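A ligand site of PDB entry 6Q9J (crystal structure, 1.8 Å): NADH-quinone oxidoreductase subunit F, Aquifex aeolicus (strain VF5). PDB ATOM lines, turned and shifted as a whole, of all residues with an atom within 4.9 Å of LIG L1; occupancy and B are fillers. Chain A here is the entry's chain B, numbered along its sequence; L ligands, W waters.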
ATOM      1  N   GLY A  67      25.733  -8.094 -25.486  1.00  0.00           N
ATOM      2  CA  GLY A  67      24.717  -9.170 -25.497  1.00  0.00           C
ATOM      3  C   GLY A  67      23.309  -8.618 -25.632  1.00  0.00           C
ATOM      4  O   GLY A  67      22.434  -9.352 -26.115  1.00  0.00           O
ATOM      5  N   GLY A  68      23.085  -7.372 -25.199  1.00  0.00           N
ATOM      6  CA  GLY A  68      21.803  -6.661 -25.383  1.00  0.00           C
ATOM      7  C   GLY A  68      21.355  -5.858 -24.167  1.00  0.00           C
ATOM      8  O   GLY A  68      20.561  -4.924 -24.369  1.00  0.00           O
ATOM      9  N   ALA A  69      21.810  -6.199 -22.956  1.00  0.00           N
ATOM     10  CA  ALA A  69      21.386  -5.502 -21.723  1.00  0.00           C
ATOM     11  C   ALA A  69      22.240  -4.247 -21.490  1.00  0.00           C
ATOM     12  O   ALA A  69      21.759  -3.347 -20.777  1.00  0.00           O
ATOM     13  CB  ALA A  69      21.418  -6.433 -20.528  1.00  0.00           C
ATOM     14  N   PHE A  71      25.077  -3.818 -19.735  1.00  0.00           N
ATOM     15  CA  PHE A  71      25.669  -3.691 -18.381  1.00  0.00           C
ATOM     16  C   PHE A  71      27.147  -3.299 -18.498  1.00  0.00           C
ATOM     17  O   PHE A  71      27.867  -3.867 -19.318  1.00  0.00           O
ATOM     18  CB  PHE A  71      25.488  -4.971 -17.570  1.00  0.00           C
ATOM     19  CG  PHE A  71      25.752  -4.782 -16.111  1.00  0.00           C
ATOM     20  CD1 PHE A  71      24.743  -4.387 -15.250  1.00  0.00           C
ATOM     21  CD2 PHE A  71      27.032  -4.950 -15.598  1.00  0.00           C
ATOM     22  CE1 PHE A  71      24.994  -4.192 -13.901  1.00  0.00           C
ATOM     23  CE2 PHE A  71      27.284  -4.747 -14.245  1.00  0.00           C
ATOM     24  CZ  PHE A  71      26.261  -4.378 -13.398  1.00  0.00           C
ATOM     25  N   LYS A  76      31.067  -5.204 -14.014  1.00  0.00           N
ATOM     26  CA  LYS A  76      30.758  -6.645 -13.847  1.00  0.00           C
ATOM     27  C   LYS A  76      32.006  -7.367 -13.328  1.00  0.00           C
ATOM     28  O   LYS A  76      31.893  -8.105 -12.326  1.00  0.00           O
ATOM     29  CB  LYS A  76      30.259  -7.284 -15.157  1.00  0.00           C
ATOM     30  CG  LYS A  76      29.652  -8.667 -14.995  1.00  0.00           C
ATOM     31  CD  LYS A  76      29.372  -9.388 -16.301  1.00  0.00           C
ATOM     32  CE  LYS A  76      28.350  -8.687 -17.165  1.00  0.00           C
ATOM     33  NZ  LYS A  76      27.829  -9.590 -18.214  1.00  0.00           N
ATOM     34  N   PHE A  79      32.798  -6.648  -9.622  1.00  0.00           N
ATOM     35  CA  PHE A  79      31.912  -7.454  -8.724  1.00  0.00           C
ATOM     36  C   PHE A  79      32.497  -8.855  -8.551  1.00  0.00           C
ATOM     37  O   PHE A  79      32.614  -9.321  -7.403  1.00  0.00           O
ATOM     38  CB  PHE A  79      30.477  -7.516  -9.250  1.00  0.00           C
ATOM     39  CG  PHE A  79      29.611  -6.335  -8.892  1.00  0.00           C
ATOM     40  CD1 PHE A  79      29.339  -6.031  -7.558  1.00  0.00           C
ATOM     41  CD2 PHE A  79      29.038  -5.540  -9.879  1.00  0.00           C
ATOM     42  CE1 PHE A  79      28.539  -4.946  -7.226  1.00  0.00           C
ATOM     43  CE2 PHE A  79      28.230  -4.457  -9.542  1.00  0.00           C
ATOM     44  CZ  PHE A  79      27.988  -4.166  -8.225  1.00  0.00           C
ATOM     45  N   GLU A  95      23.886 -16.775 -29.306  1.00  0.00           N
ATOM     46  CA  GLU A  95      23.205 -15.856 -30.260  1.00  0.00           C
ATOM     47  C   GLU A  95      22.010 -16.530 -30.946  1.00  0.00           C
ATOM     48  O   GLU A  95      22.229 -17.256 -31.941  1.00  0.00           O
ATOM     49  CB  GLU A  95      24.208 -15.360 -31.292  1.00  0.00           C
ATOM     50  CG  GLU A  95      23.587 -14.428 -32.317  1.00  0.00           C
ATOM     51  CD  GLU A  95      24.607 -13.713 -33.174  1.00  0.00           C
ATOM     52  OE1 GLU A  95      25.305 -14.398 -33.958  1.00  0.00           O
ATOM     53  OE2 GLU A  95      24.737 -12.480 -33.023  1.00  0.00           O
ATOM     54  N   SER A  96      20.800 -16.264 -30.467  1.00  0.00           N
ATOM     55  CA  SER A  96      19.546 -16.890 -30.974  1.00  0.00           C
ATOM     56  C   SER A  96      18.380 -15.889 -31.061  1.00  0.00           C
ATOM     57  O   SER A  96      17.301 -16.330 -31.456  1.00  0.00           O
ATOM     58  CB  SER A  96      19.170 -18.082 -30.129  1.00  0.00           C
ATOM     59  OG  SER A  96      20.177 -19.079 -30.183  1.00  0.00           O
ATOM     60  N   GLU A  97      18.582 -14.614 -30.707  1.00  0.00           N
ATOM     61  CA  GLU A  97      17.532 -13.566 -30.840  1.00  0.00           C
ATOM     62  C   GLU A  97      17.173 -13.418 -32.322  1.00  0.00           C
ATOM     63  O   GLU A  97      18.066 -13.261 -33.150  1.00  0.00           O
ATOM     64  CB  GLU A  97      18.005 -12.205 -30.317  1.00  0.00           C
ATOM     65  CG  GLU A  97      16.930 -11.140 -30.273  1.00  0.00           C
ATOM     66  CD  GLU A  97      15.923 -11.277 -29.139  1.00  0.00           C
ATOM     67  OE1 GLU A  97      15.915 -12.355 -28.491  1.00  0.00           O
ATOM     68  OE2 GLU A  97      15.154 -10.323 -28.902  1.00  0.00           O
ATOM     69  N   THR A 100      19.306 -11.478 -35.241  1.00  0.00           N
ATOM     70  CA  THR A 100      20.610 -11.200 -34.595  1.00  0.00           C
ATOM     71  C   THR A 100      21.656 -12.186 -35.126  1.00  0.00           C
ATOM     72  O   THR A 100      21.566 -13.396 -34.796  1.00  0.00           O
ATOM     73  CB  THR A 100      20.473 -11.210 -33.071  1.00  0.00           C
ATOM     74  OG1 THR A 100      19.312 -10.457 -32.736  1.00  0.00           O
ATOM     75  CG2 THR A 100      21.691 -10.642 -32.367  1.00  0.00           C
ATOM     76  N   ASP A 103      27.319 -11.795 -33.865  1.00  0.00           N
ATOM     77  CA  ASP A 103      28.390 -12.553 -33.161  1.00  0.00           C
ATOM     78  C   ASP A 103      29.026 -13.592 -34.087  1.00  0.00           C
ATOM     79  O   ASP A 103      30.254 -13.789 -34.020  1.00  0.00           O
ATOM     80  CB  ASP A 103      27.885 -13.256 -31.905  1.00  0.00           C
ATOM     81  CG  ASP A 103      27.349 -12.309 -30.841  1.00  0.00           C
ATOM     82  OD1 ASP A 103      27.654 -11.103 -30.928  1.00  0.00           O
ATOM     83  OD2 ASP A 103      26.631 -12.785 -29.953  1.00  0.00           O
ATOM     84  N   TYR A 180      16.789 -21.500 -27.029  1.00  0.00           N
ATOM     85  CA  TYR A 180      16.994 -20.030 -26.906  1.00  0.00           C
ATOM     86  C   TYR A 180      17.343 -19.669 -25.457  1.00  0.00           C
ATOM     87  O   TYR A 180      18.170 -18.764 -25.256  1.00  0.00           O
ATOM     88  CB  TYR A 180      15.713 -19.331 -27.355  1.00  0.00           C
ATOM     89  CG  TYR A 180      15.590 -17.853 -27.082  1.00  0.00           C
ATOM     90  CD1 TYR A 180      16.280 -16.905 -27.827  1.00  0.00           C
ATOM     91  CD2 TYR A 180      14.665 -17.396 -26.156  1.00  0.00           C
ATOM     92  CE1 TYR A 180      16.091 -15.552 -27.623  1.00  0.00           C
ATOM     93  CE2 TYR A 180      14.474 -16.040 -25.935  1.00  0.00           C
ATOM     94  CZ  TYR A 180      15.183 -15.120 -26.666  1.00  0.00           C
ATOM     95  OH  TYR A 180      14.962 -13.787 -26.445  1.00  0.00           O
ATOM     96  N   GLU A 185      22.135 -16.212 -18.991  1.00  0.00           N
ATOM     97  CA  GLU A 185      23.481 -16.535 -18.421  1.00  0.00           C
ATOM     98  C   GLU A 185      23.373 -17.662 -17.386  1.00  0.00           C
ATOM     99  O   GLU A 185      24.305 -18.481 -17.330  1.00  0.00           O
ATOM    100  CB  GLU A 185      24.133 -15.290 -17.822  1.00  0.00           C
ATOM    101  CG  GLU A 185      23.311 -14.606 -16.759  1.00  0.00           C
ATOM    102  CD  GLU A 185      23.972 -13.398 -16.129  1.00  0.00           C
ATOM    103  OE1 GLU A 185      25.080 -13.036 -16.569  1.00  0.00           O
ATOM    104  OE2 GLU A 185      23.384 -12.836 -15.188  1.00  0.00           O
ATOM    105  N   TYR A 205      23.807 -13.050  -8.706  1.00  0.00           N
ATOM    106  CA  TYR A 205      24.340 -12.961 -10.085  1.00  0.00           C
ATOM    107  C   TYR A 205      25.528 -13.903 -10.196  1.00  0.00           C
ATOM    108  O   TYR A 205      26.156 -14.259  -9.202  1.00  0.00           O
ATOM    109  CB  TYR A 205      24.649 -11.507 -10.450  1.00  0.00           C
ATOM    110  CG  TYR A 205      23.405 -10.649 -10.520  1.00  0.00           C
ATOM    111  CD1 TYR A 205      22.584 -10.670 -11.641  1.00  0.00           C
ATOM    112  CD2 TYR A 205      23.012  -9.878  -9.445  1.00  0.00           C
ATOM    113  CE1 TYR A 205      21.435  -9.915 -11.696  1.00  0.00           C
ATOM    114  CE2 TYR A 205      21.861  -9.119  -9.484  1.00  0.00           C
ATOM    115  CZ  TYR A 205      21.056  -9.136 -10.615  1.00  0.00           C
ATOM    116  OH  TYR A 205      19.926  -8.399 -10.653  1.00  0.00           O
ATOM    117  N   PRO A 206      25.846 -14.361 -11.430  1.00  0.00           N
ATOM    118  CA  PRO A 206      26.956 -15.280 -11.645  1.00  0.00           C
ATOM    119  C   PRO A 206      28.272 -14.815 -10.997  1.00  0.00           C
ATOM    120  O   PRO A 206      29.000 -15.652 -10.509  1.00  0.00           O
ATOM    121  CB  PRO A 206      27.063 -15.336 -13.173  1.00  0.00           C
ATOM    122  CG  PRO A 206      25.642 -15.097 -13.636  1.00  0.00           C
ATOM    123  CD  PRO A 206      25.116 -14.058 -12.677  1.00  0.00           C
ATOM    124  N   VAL A 207      28.531 -13.502 -10.986  1.00  0.00           N
ATOM    125  CA  VAL A 207      29.794 -12.912 -10.447  1.00  0.00           C
ATOM    126  C   VAL A 207      29.923 -13.250  -8.955  1.00  0.00           C
ATOM    127  O   VAL A 207      31.063 -13.263  -8.478  1.00  0.00           O
ATOM    128  CB  VAL A 207      29.895 -11.397 -10.697  1.00  0.00           C
ATOM    129  CG1 VAL A 207      30.042 -11.085 -12.183  1.00  0.00           C
ATOM    130  CG2 VAL A 207      28.739 -10.627 -10.087  1.00  0.00           C
ATOM    131  N   VAL A 218      29.989 -13.902 -17.163  1.00  0.00           N
ATOM    132  CA  VAL A 218      29.440 -14.232 -18.503  1.00  0.00           C
ATOM    133  C   VAL A 218      29.486 -12.951 -19.326  1.00  0.00           C
ATOM    134  O   VAL A 218      28.950 -11.921 -18.853  1.00  0.00           O
ATOM    135  CB  VAL A 218      28.011 -14.812 -18.426  1.00  0.00           C
ATOM    136  CG1 VAL A 218      27.489 -15.165 -19.811  1.00  0.00           C
ATOM    137  CG2 VAL A 218      27.960 -16.029 -17.502  1.00  0.00           C
ATOM    138  N   ASN A 220      29.218 -11.566 -23.621  1.00  0.00           N
ATOM    139  CA  ASN A 220      28.846 -11.791 -25.034  1.00  0.00           C
ATOM    140  C   ASN A 220      30.107 -11.741 -25.910  1.00  0.00           C
ATOM    141  O   ASN A 220      31.041 -10.986 -25.589  1.00  0.00           O
ATOM    142  CB  ASN A 220      27.807 -10.745 -25.450  1.00  0.00           C
ATOM    143  CG  ASN A 220      27.501 -10.749 -26.931  1.00  0.00           C
ATOM    144  OD1 ASN A 220      28.008  -9.910 -27.668  1.00  0.00           O
ATOM    145  ND2 ASN A 220      26.676 -11.695 -27.355  1.00  0.00           N
ATOM    146  N   LEU A 297      12.358  -7.927 -28.988  1.00  0.00           N
ATOM    147  CA  LEU A 297      12.354  -7.119 -27.725  1.00  0.00           C
ATOM    148  C   LEU A 297      11.453  -5.874 -27.870  1.00  0.00           C
ATOM    149  O   LEU A 297      10.599  -5.661 -26.982  1.00  0.00           O
ATOM    150  CB  LEU A 297      13.798  -6.711 -27.399  1.00  0.00           C
ATOM    151  CG  LEU A 297      14.011  -6.003 -26.070  1.00  0.00           C
ATOM    152  CD1 LEU A 297      13.620  -6.891 -24.905  1.00  0.00           C
ATOM    153  CD2 LEU A 297      15.462  -5.552 -25.936  1.00  0.00           C
ATOM    154  N   GLY A 318      19.258  -2.600 -26.854  1.00  0.00           N
ATOM    155  CA  GLY A 318      19.191  -4.036 -27.183  1.00  0.00           C
ATOM    156  C   GLY A 318      20.471  -4.511 -27.851  1.00  0.00           C
ATOM    157  O   GLY A 318      21.551  -4.025 -27.506  1.00  0.00           O
ATOM    158  N   THR A 319      20.341  -5.445 -28.799  1.00  0.00           N
ATOM    159  CA  THR A 319      21.459  -6.091 -29.516  1.00  0.00           C
ATOM    160  C   THR A 319      21.973  -5.194 -30.642  1.00  0.00           C
ATOM    161  O   THR A 319      23.047  -5.505 -31.179  1.00  0.00           O
ATOM    162  CB  THR A 319      21.012  -7.456 -30.076  1.00  0.00           C
ATOM    163  OG1 THR A 319      19.869  -7.213 -30.887  1.00  0.00           O
ATOM    164  CG2 THR A 319      20.660  -8.464 -29.008  1.00  0.00           C
ATOM    165  N   GLY A 394      14.563 -12.861 -17.996  1.00  0.00           N
ATOM    166  CA  GLY A 394      14.186 -11.800 -18.947  1.00  0.00           C
ATOM    167  C   GLY A 394      13.158 -12.252 -19.961  1.00  0.00           C
ATOM    168  O   GLY A 394      12.497 -11.355 -20.505  1.00  0.00           O
HETATM  169  P1  LIG L   1      20.240  -7.957 -17.097  1.00  0.00           P
HETATM  170  O1  LIG L   1      20.100  -6.494 -17.322  1.00  0.00           O
HETATM  171  O2  LIG L   1      19.394  -8.539 -15.986  1.00  0.00           O
HETATM  172  O3  LIG L   1      21.772  -8.379 -16.803  1.00  0.00           O
HETATM  173  C1  LIG L   1      22.814  -8.016 -17.733  1.00  0.00           C
HETATM  174  C2  LIG L   1      24.154  -8.466 -17.200  1.00  0.00           C
HETATM  175  O4  LIG L   1      24.527  -7.647 -16.077  1.00  0.00           O
HETATM  176  C3  LIG L   1      24.214  -9.919 -16.714  1.00  0.00           C
HETATM  177  O5  LIG L   1      25.479 -10.487 -16.987  1.00  0.00           O
HETATM  178  C4  LIG L   1      23.963  -9.762 -15.201  1.00  0.00           C
HETATM  179  O6  LIG L   1      24.546 -10.825 -14.446  1.00  0.00           O
HETATM  180  C5  LIG L   1      24.691  -8.455 -14.924  1.00  0.00           C
HETATM  181  N1  LIG L   1      24.164  -7.725 -13.770  1.00  0.00           N
HETATM  182  C6  LIG L   1      22.986  -7.037 -13.681  1.00  0.00           C
HETATM  183  N2  LIG L   1      22.755  -6.521 -12.494  1.00  0.00           N
HETATM  184  C7  LIG L   1      23.853  -6.903 -11.745  1.00  0.00           C
HETATM  185  C8  LIG L   1      24.220  -6.682 -10.398  1.00  0.00           C
HETATM  186  N3  LIG L   1      23.459  -6.007  -9.526  1.00  0.00           N
HETATM  187  N4  LIG L   1      25.387  -7.200  -9.969  1.00  0.00           N
HETATM  188  C9  LIG L   1      26.146  -7.890 -10.833  1.00  0.00           C
HETATM  189  N5  LIG L   1      25.904  -8.168 -12.117  1.00  0.00           N
HETATM  190  C10 LIG L   1      24.740  -7.641 -12.516  1.00  0.00           C
HETATM  191  O7  LIG L   1      19.861  -8.736 -18.429  1.00  0.00           O
HETATM  192  P2  LIG L   1      19.723 -10.261 -18.834  1.00  0.00           P
HETATM  193  O8  LIG L   1      18.392 -10.757 -18.309  1.00  0.00           O
HETATM  194  O9  LIG L   1      20.933 -11.071 -18.511  1.00  0.00           O
HETATM  195  O10 LIG L   1      19.582 -10.105 -20.436  1.00  0.00           O
HETATM  196  C11 LIG L   1      18.508  -9.446 -21.139  1.00  0.00           C
HETATM  197  C12 LIG L   1      18.971  -9.111 -22.533  1.00  0.00           C
HETATM  198  O11 LIG L   1      19.288 -10.320 -23.257  1.00  0.00           O
HETATM  199  C13 LIG L   1      17.958  -8.374 -23.403  1.00  0.00           C
HETATM  200  O12 LIG L   1      18.208  -6.975 -23.362  1.00  0.00           O
HETATM  201  C14 LIG L   1      18.177  -8.939 -24.819  1.00  0.00           C
HETATM  202  O13 LIG L   1      18.579  -7.923 -25.734  1.00  0.00           O
HETATM  203  C15 LIG L   1      19.328  -9.944 -24.627  1.00  0.00           C
HETATM  204  N6  LIG L   1      19.223 -11.144 -25.451  1.00  0.00           N
HETATM  205  C16 LIG L   1      20.160 -11.409 -26.483  1.00  0.00           C
HETATM  206  C17 LIG L   1      20.103 -12.492 -27.269  1.00  0.00           C
HETATM  207  C18 LIG L   1      21.120 -12.651 -28.335  1.00  0.00           C
HETATM  208  O14 LIG L   1      20.962 -13.509 -29.213  1.00  0.00           O
HETATM  209  N7  LIG L   1      22.183 -11.857 -28.306  1.00  0.00           N
HETATM  210  C19 LIG L   1      19.019 -13.505 -27.088  1.00  0.00           C
HETATM  211  C20 LIG L   1      18.083 -13.125 -25.994  1.00  0.00           C
HETATM  212  C21 LIG L   1      18.213 -12.035 -25.264  1.00  0.00           C
HETATM  213  N1  LG2 L   2      23.351 -12.969 -24.155  1.00  0.00           N
HETATM  214  C1  LG2 L   2      24.188 -13.351 -25.155  1.00  0.00           C
HETATM  215  O1  LG2 L   2      25.344 -12.922 -25.210  1.00  0.00           O
HETATM  216  N2  LG2 L   2      23.764 -14.288 -26.095  1.00  0.00           N
HETATM  217  C2  LG2 L   2      22.547 -14.921 -26.104  1.00  0.00           C
HETATM  218  O2  LG2 L   2      22.277 -15.733 -26.995  1.00  0.00           O
HETATM  219  C3  LG2 L   2      21.662 -14.525 -25.019  1.00  0.00           C
HETATM  220  N3  LG2 L   2      20.496 -15.104 -24.924  1.00  0.00           N
HETATM  221  C4  LG2 L   2      19.652 -14.712 -23.874  1.00  0.00           C
HETATM  222  C5  LG2 L   2      18.390 -15.294 -23.756  1.00  0.00           C
HETATM  223  C6  LG2 L   2      17.492 -14.892 -22.780  1.00  0.00           C
HETATM  224  C7  LG2 L   2      16.134 -15.535 -22.706  1.00  0.00           C
HETATM  225  C8  LG2 L   2      17.873 -13.887 -21.870  1.00  0.00           C
HETATM  226  C9  LG2 L   2      16.913 -13.362 -20.831  1.00  0.00           C
HETATM  227  C10 LG2 L   2      19.143 -13.332 -21.952  1.00  0.00           C
HETATM  228  C11 LG2 L   2      20.037 -13.725 -22.948  1.00  0.00           C
HETATM  229  N4  LG2 L   2      21.329 -13.147 -23.078  1.00  0.00           N
HETATM  230  C12 LG2 L   2      22.155 -13.532 -24.097  1.00  0.00           C
HETATM  231  C13 LG2 L   2      21.838 -12.161 -22.118  1.00  0.00           C
HETATM  232  C14 LG2 L   2      22.663 -12.812 -21.017  1.00  0.00           C
HETATM  233  O3  LG2 L   2      21.809 -13.267 -19.967  1.00  0.00           O
HETATM  234  C15 LG2 L   2      23.719 -11.857 -20.451  1.00  0.00           C
HETATM  235  O4  LG2 L   2      23.114 -10.617 -20.104  1.00  0.00           O
HETATM  236  C16 LG2 L   2      24.913 -11.564 -21.358  1.00  0.00           C
HETATM  237  O5  LG2 L   2      25.380 -12.759 -21.981  1.00  0.00           O
HETATM  238  C17 LG2 L   2      26.008 -10.883 -20.574  1.00  0.00           C
HETATM  239  O6  LG2 L   2      27.040 -10.450 -21.466  1.00  0.00           O
HETATM  240  P1  LG2 L   2      27.278  -8.916 -21.819  1.00  0.00           P
HETATM  241  O7  LG2 L   2      26.202  -8.449 -22.753  1.00  0.00           O
HETATM  242  O8  LG2 L   2      27.294  -8.123 -20.498  1.00  0.00           O
HETATM  243  O9  LG2 L   2      28.680  -8.863 -22.428  1.00  0.00           O
HETATM  244  O   HOH W   1      19.194 -10.735 -14.571  1.00  0.00           O
HETATM  245  O   HOH W   2      20.538  -5.027 -12.419  1.00  0.00           O
HETATM  246  O   HOH W   3      15.077 -11.058 -24.250  1.00  0.00           O
HETATM  247  O   HOH W   4      20.793  -5.164  -9.744  1.00  0.00           O
HETATM  248  O   HOH W   5      21.308  -4.354 -16.521  1.00  0.00           O
HETATM  249  O   HOH W   6      17.399 -12.972 -17.152  1.00  0.00           O
HETATM  250  O   HOH W   7      16.946  -5.853 -21.368  1.00  0.00           O
HETATM  251  O   HOH W   8      20.667 -12.406 -16.046  1.00  0.00           O
HETATM  252  O   HOH W   9      16.252  -9.109 -17.987  1.00  0.00           O
HETATM  253  O   HOH W  10      26.895 -11.000 -13.354  1.00  0.00           O
HETATM  254  O   HOH W  11      16.930  -8.397 -27.924  1.00  0.00           O
HETATM  255  O   HOH W  12      25.721  -7.306  -7.142  1.00  0.00           O
HETATM  256  O   HOH W  13      24.297 -11.525 -30.359  1.00  0.00           O
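NZ of Lys 76 is in hydrogen-bond range of O of Val 218. The side-chain carboxylate (OE1) of Glu 97 sits at hydrogen-bond distance from the side-chain hydroxyl (OH) of Tyr 180 (2.7 Å). The backbone carbonyl oxygen of Glu 97 is in hydrogen-bond range of the side-chain hydroxyl of Thr 100, 3.1 Å away. OE2 of Glu 95 is in hydrogen-bond range of N of Asp 103 (2.8 Å).
An oxygen (O9) of LIG L1 is in hydrogen-bond range of an oxygen (O4) of LG2 L2 (2.7 Å).
O1 of LG2 L2 sits at hydrogen-bond distance from ND2 of Asn 220 (2.8 Å). The side-chain amino group (NZ) of Lys 76 is in salt-bridge range of an oxygen (O8) of LG2 L2 (2.8 Å). O12 of LIG L1 is in hydrogen-bond range of O of Gly 68 (3.3 Å). The backbone NH (N) of Ser 96 sits at hydrogen-bond distance from an oxygen (O14) of LIG L1, at 3.0 Å. The side-chain amino group (NZ) of Lys 76 is in hydrogen-bond range of an oxygen (O5) of LIG L1 (2.8 Å). The backbone NH (N) of Glu 97 is in hydrogen-bond range of an oxygen (O14) of LIG L1 (3.0 Å). O3 of LG2 L2 sits at hydrogen-bond distance from N of Glu 185 (3.1 Å). N of Gly 67 is in hydrogen-bond range of O7 of LG2 L2 (2.8 Å). The backbone carbonyl oxygen (O) of Gly 67 sits close to a nitrogen (N7) of LIG L1 (3.3 Å). N of Asn 220 lies within hydrogen-bond range of O9 of LG2 L2 (3.0 Å). N of Glu 95 lies within hydrogen-bond range of O2 of LG2 L2 (3.0 Å). OE2 of Glu 185 sits at hydrogen-bond distance from O6 of LIG L1 (2.4 Å).
Water W6 bridges an oxygen (O8) of LIG L1 (2.7 Å) and the backbone NH of Gly 394 (3.0 Å). Water W11 lies within hydrogen-bond range of O13 of LIG L1 and OE2 of Glu 97. Water W4 lies within hydrogen-bond range of N3 of LIG L1 (2.8 Å) and OH of Tyr 205 (3.5 Å). Water W8 bridges O9 of LIG L1 and OE2 of Glu 185. Water W13 lies within hydrogen-bond range of OD2 of Asp 103 (2.7 Å), OE2 of Glu 95 (2.9 Å) and N7 of LIG L1 (3.0 Å).
Residues that only touch LIG L1: Ala 69 (3.5 Å), Phe 71 (3.1 Å), Phe 79 (3.8 Å), Glu 95 (3.4 Å), Tyr 180 (3.2 Å), Tyr 205 (3.4 Å), Pro 206 (3.7 Å), Val 207 (3.8 Å), Leu 297 (3.9 Å) and Thr 319 (3.8 Å). Hydrophobic or aromatic side chains that line LIG L1: Ala 69, Phe 71, Phe 79, Tyr 180, Tyr 205, Pro 206, Val 207 and Leu 297.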
